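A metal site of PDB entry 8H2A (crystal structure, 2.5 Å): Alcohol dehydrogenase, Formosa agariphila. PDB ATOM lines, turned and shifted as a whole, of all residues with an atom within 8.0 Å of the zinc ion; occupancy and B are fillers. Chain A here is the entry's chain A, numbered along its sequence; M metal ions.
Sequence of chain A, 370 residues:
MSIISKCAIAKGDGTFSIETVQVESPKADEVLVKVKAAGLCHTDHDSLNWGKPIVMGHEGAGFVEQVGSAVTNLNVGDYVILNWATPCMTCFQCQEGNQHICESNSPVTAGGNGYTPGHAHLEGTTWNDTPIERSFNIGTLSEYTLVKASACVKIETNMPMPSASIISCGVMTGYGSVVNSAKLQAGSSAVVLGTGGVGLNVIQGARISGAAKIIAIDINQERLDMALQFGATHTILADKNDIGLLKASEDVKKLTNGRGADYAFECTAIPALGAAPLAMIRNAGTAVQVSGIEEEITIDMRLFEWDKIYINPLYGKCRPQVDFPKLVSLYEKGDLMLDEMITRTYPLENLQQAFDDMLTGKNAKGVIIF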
ATOM      1  N   ALA A  85      21.708  33.452 -17.628  1.00  0.00           N
ATOM      2  CA  ALA A  85      21.939  32.634 -16.445  1.00  0.00           C
ATOM      3  C   ALA A  85      21.217  31.298 -16.585  1.00  0.00           C
ATOM      4  O   ALA A  85      21.769  30.251 -16.238  1.00  0.00           O
ATOM      5  CB  ALA A  85      21.481  33.388 -15.197  1.00  0.00           C
ATOM      6  N   THR A  86      20.020  31.329 -17.178  1.00  0.00           N
ATOM      7  CA  THR A  86      19.077  30.218 -17.330  1.00  0.00           C
ATOM      8  C   THR A  86      18.994  29.374 -16.065  1.00  0.00           C
ATOM      9  O   THR A  86      19.111  28.140 -16.133  1.00  0.00           O
ATOM     10  CB  THR A  86      19.428  29.366 -18.555  1.00  0.00           C
ATOM     11  OG1 THR A  86      20.816  28.993 -18.542  1.00  0.00           O
ATOM     12  CG2 THR A  86      19.135  30.142 -19.811  1.00  0.00           C
ATOM     13  N   PRO A  87      18.715  29.989 -14.908  1.00  0.00           N
ATOM     14  CA  PRO A  87      18.916  29.293 -13.620  1.00  0.00           C
ATOM     15  C   PRO A  87      17.921  28.166 -13.413  1.00  0.00           C
ATOM     16  O   PRO A  87      16.718  28.324 -13.633  1.00  0.00           O
ATOM     17  CB  PRO A  87      18.725  30.408 -12.596  1.00  0.00           C
ATOM     18  CG  PRO A  87      17.821  31.429 -13.314  1.00  0.00           C
ATOM     19  CD  PRO A  87      18.260  31.386 -14.729  1.00  0.00           C
ATOM     20  N   CYS A  88      18.445  27.016 -12.965  1.00  0.00           N
ATOM     21  CA  CYS A  88      17.601  25.887 -12.609  1.00  0.00           C
ATOM     22  C   CYS A  88      16.969  26.071 -11.231  1.00  0.00           C
ATOM     23  O   CYS A  88      16.061  25.307 -10.880  1.00  0.00           O
ATOM     24  CB  CYS A  88      18.401  24.584 -12.604  1.00  0.00           C
ATOM     25  SG  CYS A  88      19.323  24.294 -11.062  1.00  0.00           S
ATOM     26  N   MET A  89      17.463  27.038 -10.457  1.00  0.00           N
ATOM     27  CA  MET A  89      16.951  27.428  -9.148  1.00  0.00           C
ATOM     28  C   MET A  89      17.089  26.396  -8.045  1.00  0.00           C
ATOM     29  O   MET A  89      16.904  26.734  -6.871  1.00  0.00           O
ATOM     30  CB  MET A  89      15.488  27.816  -9.203  1.00  0.00           C
ATOM     31  CG  MET A  89      15.151  29.054  -9.972  1.00  0.00           C
ATOM     32  SD  MET A  89      16.105  30.456  -9.353  1.00  0.00           S
ATOM     33  CE  MET A  89      15.393  31.817 -10.260  1.00  0.00           C
ATOM     34  N   THR A  90      17.377  25.130  -8.354  1.00  0.00           N
ATOM     35  CA  THR A  90      17.350  24.093  -7.330  1.00  0.00           C
ATOM     36  C   THR A  90      18.726  23.558  -6.942  1.00  0.00           C
ATOM     37  O   THR A  90      18.851  22.956  -5.878  1.00  0.00           O
ATOM     38  CB  THR A  90      16.492  22.891  -7.770  1.00  0.00           C
ATOM     39  OG1 THR A  90      16.944  22.414  -9.048  1.00  0.00           O
ATOM     40  CG2 THR A  90      15.015  23.308  -7.859  1.00  0.00           C
ATOM     41  N   CYS A  91      19.743  23.771  -7.770  1.00  0.00           N
ATOM     42  CA  CYS A  91      21.019  23.146  -7.535  1.00  0.00           C
ATOM     43  C   CYS A  91      21.742  23.823  -6.383  1.00  0.00           C
ATOM     44  O   CYS A  91      21.316  24.862  -5.859  1.00  0.00           O
ATOM     45  CB  CYS A  91      21.868  23.173  -8.796  1.00  0.00           C
ATOM     46  SG  CYS A  91      22.541  24.818  -9.180  1.00  0.00           S
ATOM     47  N   PHE A  92      22.866  23.218  -5.993  1.00  0.00           N
ATOM     48  CA  PHE A  92      23.696  23.728  -4.925  1.00  0.00           C
ATOM     49  C   PHE A  92      24.042  25.207  -5.149  1.00  0.00           C
ATOM     50  O   PHE A  92      23.923  26.025  -4.236  1.00  0.00           O
ATOM     51  CB  PHE A  92      24.968  22.882  -4.813  1.00  0.00           C
ATOM     52  CG  PHE A  92      26.023  23.462  -3.904  1.00  0.00           C
ATOM     53  CD1 PHE A  92      26.916  24.422  -4.374  1.00  0.00           C
ATOM     54  CD2 PHE A  92      26.112  23.057  -2.577  1.00  0.00           C
ATOM     55  CE1 PHE A  92      27.876  24.983  -3.537  1.00  0.00           C
ATOM     56  CE2 PHE A  92      27.082  23.600  -1.748  1.00  0.00           C
ATOM     57  CZ  PHE A  92      27.969  24.560  -2.239  1.00  0.00           C
ATOM     58  N   GLN A  93      24.508  25.563  -6.355  1.00  0.00           N
ATOM     59  CA  GLN A  93      24.952  26.930  -6.541  1.00  0.00           C
ATOM     60  C   GLN A  93      23.769  27.885  -6.520  1.00  0.00           C
ATOM     61  O   GLN A  93      23.853  28.969  -5.920  1.00  0.00           O
ATOM     62  CB  GLN A  93      25.776  27.066  -7.825  1.00  0.00           C
ATOM     63  CG  GLN A  93      27.147  26.387  -7.713  1.00  0.00           C
ATOM     64  CD  GLN A  93      28.181  27.226  -6.970  1.00  0.00           C
ATOM     65  OE1 GLN A  93      27.843  28.251  -6.346  1.00  0.00           O
ATOM     66  NE2 GLN A  93      29.429  26.802  -7.009  1.00  0.00           N
ATOM     67  N   CYS A  94      22.641  27.468  -7.097  1.00  0.00           N
ATOM     68  CA  CYS A  94      21.425  28.280  -7.047  1.00  0.00           C
ATOM     69  C   CYS A  94      20.899  28.446  -5.627  1.00  0.00           C
ATOM     70  O   CYS A  94      20.294  29.482  -5.295  1.00  0.00           O
ATOM     71  CB  CYS A  94      20.335  27.660  -7.929  1.00  0.00           C
ATOM     72  SG  CYS A  94      20.483  27.955  -9.713  1.00  0.00           S
ATOM     73  N   GLN A  95      21.077  27.444  -4.778  1.00  0.00           N
ATOM     74  CA  GLN A  95      20.606  27.594  -3.408  1.00  0.00           C
ATOM     75  C   GLN A  95      21.542  28.468  -2.565  1.00  0.00           C
ATOM     76  O   GLN A  95      21.128  28.953  -1.505  1.00  0.00           O
ATOM     77  CB  GLN A  95      20.395  26.222  -2.775  1.00  0.00           C
ATOM     78  CG  GLN A  95      19.214  25.538  -3.392  1.00  0.00           C
ATOM     79  CD  GLN A  95      18.560  24.523  -2.499  1.00  0.00           C
ATOM     80  OE1 GLN A  95      18.287  24.769  -1.322  1.00  0.00           O
ATOM     81  NE2 GLN A  95      18.252  23.364  -3.068  1.00  0.00           N
ATOM     82  N   ASN A  98      23.832  31.815  -5.973  1.00  0.00           N
ATOM     83  CA  ASN A  98      24.711  31.865  -7.141  1.00  0.00           C
ATOM     84  C   ASN A  98      24.026  31.179  -8.328  1.00  0.00           C
ATOM     85  O   ASN A  98      24.453  30.138  -8.824  1.00  0.00           O
ATOM     86  CB  ASN A  98      26.048  31.220  -6.807  1.00  0.00           C
ATOM     87  CG  ASN A  98      26.765  31.928  -5.697  1.00  0.00           C
ATOM     88  OD1 ASN A  98      26.602  33.137  -5.525  1.00  0.00           O
ATOM     89  ND2 ASN A  98      27.586  31.195  -4.938  1.00  0.00           N
ATOM     90  N   GLN A  99      22.944  31.796  -8.789  1.00  0.00           N
ATOM     91  CA  GLN A  99      22.334  31.356 -10.036  1.00  0.00           C
ATOM     92  C   GLN A  99      23.194  31.672 -11.263  1.00  0.00           C
ATOM     93  O   GLN A  99      22.945  31.103 -12.330  1.00  0.00           O
ATOM     94  CB  GLN A  99      20.954  31.985 -10.229  1.00  0.00           C
ATOM     95  CG  GLN A  99      20.151  32.195  -8.971  1.00  0.00           C
ATOM     96  CD  GLN A  99      18.829  32.923  -9.237  1.00  0.00           C
ATOM     97  OE1 GLN A  99      18.567  33.371 -10.352  1.00  0.00           O
ATOM     98  NE2 GLN A  99      17.981  33.029  -8.211  1.00  0.00           N
ATOM     99  N   HIS A 100      24.171  32.576 -11.147  1.00  0.00           N
ATOM    100  CA  HIS A 100      25.031  32.889 -12.290  1.00  0.00           C
ATOM    101  C   HIS A 100      26.042  31.792 -12.579  1.00  0.00           C
ATOM    102  O   HIS A 100      26.731  31.865 -13.613  1.00  0.00           O
ATOM    103  CB  HIS A 100      25.758  34.201 -12.037  1.00  0.00           C
ATOM    104  CG  HIS A 100      26.528  34.205 -10.751  1.00  0.00           C
ATOM    105  ND1 HIS A 100      25.911  34.243  -9.515  1.00  0.00           N
ATOM    106  CD2 HIS A 100      27.849  34.166 -10.512  1.00  0.00           C
ATOM    107  CE1 HIS A 100      26.837  34.226  -8.569  1.00  0.00           C
ATOM    108  NE2 HIS A 100      28.027  34.182  -9.151  1.00  0.00           N
ATOM    109  N   ILE A 101      26.149  30.784 -11.731  1.00  0.00           N
ATOM    110  CA  ILE A 101      27.170  29.755 -11.848  1.00  0.00           C
ATOM    111  C   ILE A 101      26.459  28.408 -11.677  1.00  0.00           C
ATOM    112  O   ILE A 101      27.023  27.429 -11.172  1.00  0.00           O
ATOM    113  CB  ILE A 101      28.318  29.992 -10.826  1.00  0.00           C
ATOM    114  CG1 ILE A 101      29.491  29.033 -11.031  1.00  0.00           C
ATOM    115  CG2 ILE A 101      27.831  29.868  -9.390  1.00  0.00           C
ATOM    116  CD1 ILE A 101      30.424  29.461 -12.069  1.00  0.00           C
ATOM    117  N   CYS A 102      25.202  28.377 -12.131  1.00  0.00           N
ATOM    118  CA  CYS A 102      24.353  27.197 -12.053  1.00  0.00           C
ATOM    119  C   CYS A 102      25.061  25.946 -12.557  1.00  0.00           C
ATOM    120  O   CYS A 102      25.588  25.911 -13.667  1.00  0.00           O
ATOM    121  CB  CYS A 102      23.077  27.455 -12.863  1.00  0.00           C
ATOM    122  SG  CYS A 102      21.793  26.202 -12.748  1.00  0.00           S
ATOM    123  N   GLU A 103      25.029  24.886 -11.747  1.00  0.00           N
ATOM    124  CA  GLU A 103      25.769  23.676 -12.079  1.00  0.00           C
ATOM    125  C   GLU A 103      25.155  22.870 -13.214  1.00  0.00           C
ATOM    126  O   GLU A 103      25.860  22.075 -13.825  1.00  0.00           O
ATOM    127  CB  GLU A 103      25.908  22.812 -10.813  1.00  0.00           C
ATOM    128  CG  GLU A 103      26.517  23.606  -9.657  1.00  0.00           C
ATOM    129  CD  GLU A 103      27.123  22.746  -8.558  1.00  0.00           C
ATOM    130  OE1 GLU A 103      26.560  21.683  -8.190  1.00  0.00           O
ATOM    131  OE2 GLU A 103      28.187  23.161  -8.060  1.00  0.00           O
ATOM    132  N   SER A 104      23.863  23.041 -13.518  1.00  0.00           N
ATOM    133  CA  SER A 104      23.198  22.228 -14.534  1.00  0.00           C
ATOM    134  C   SER A 104      22.699  22.984 -15.743  1.00  0.00           C
ATOM    135  O   SER A 104      22.534  22.363 -16.797  1.00  0.00           O
ATOM    136  CB  SER A 104      21.999  21.478 -13.937  1.00  0.00           C
ATOM    137  OG  SER A 104      22.430  20.394 -13.132  1.00  0.00           O
ATOM    138  N   ASN A 105      22.428  24.284 -15.652  1.00  0.00           N
ATOM    139  CA  ASN A 105      21.870  25.003 -16.785  1.00  0.00           C
ATOM    140  C   ASN A 105      22.757  26.119 -17.319  1.00  0.00           C
ATOM    141  O   ASN A 105      22.500  26.609 -18.431  1.00  0.00           O
ATOM    142  CB  ASN A 105      20.495  25.579 -16.428  1.00  0.00           C
ATOM    143  CG  ASN A 105      19.476  24.515 -16.169  1.00  0.00           C
ATOM    144  OD1 ASN A 105      19.823  23.360 -15.856  1.00  0.00           O
ATOM    145  ND2 ASN A 105      18.204  24.868 -16.288  1.00  0.00           N
ATOM    146  N   SER A 106      23.784  26.555 -16.579  1.00  0.00           N
ATOM    147  CA  SER A 106      24.654  27.613 -17.059  1.00  0.00           C
ATOM    148  C   SER A 106      25.299  27.215 -18.382  1.00  0.00           C
ATOM    149  O   SER A 106      25.783  26.091 -18.527  1.00  0.00           O
ATOM    150  CB  SER A 106      25.745  27.909 -16.035  1.00  0.00           C
ATOM    151  OG  SER A 106      26.790  28.693 -16.589  1.00  0.00           O
HETATM  152 ZN    ZN M   1      21.001  25.842 -10.602  1.00  0.00          ZN
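SG of Cys 102 sits close to N of Asn 105 (3.5 Å).
N of Thr 90 sits close to SG of Cys 88, at 3.4 Å.
The side-chain sulfur (SG) of Cys 91 lies close to the backbone NH (N) of Glu 103 (3.6 Å).
The side-chain sulfur of Cys 91 lies close to the backbone NH of Gln 93, 3.5 Å away.
SG of Cys 94 lies close to N of Met 89.
The side-chain amide nitrogen of Gln 99 lies within hydrogen-bond range of the side-chain sulfur of Met 89 (3.4 Å).
N of Met 89 touches the zinc ion, at 3.7 Å.
Five residues have an atom within 4 Å of the zinc ion: Cys 88, Met 89, Cys 91, Cys 94 and Cys 102.
SG of Cys 102 is bound to the zinc ion (2.3 Å).
The side-chain sulfur (SG) of Cys 88 is bound to the zinc ion, at 2.3 Å.
SG of Cys 91 binds the zinc ion, 2.3 Å away.
SG of Cys 94 is bound to the zinc ion (2.4 Å).
The zinc ion has four donor atoms within binding distance.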
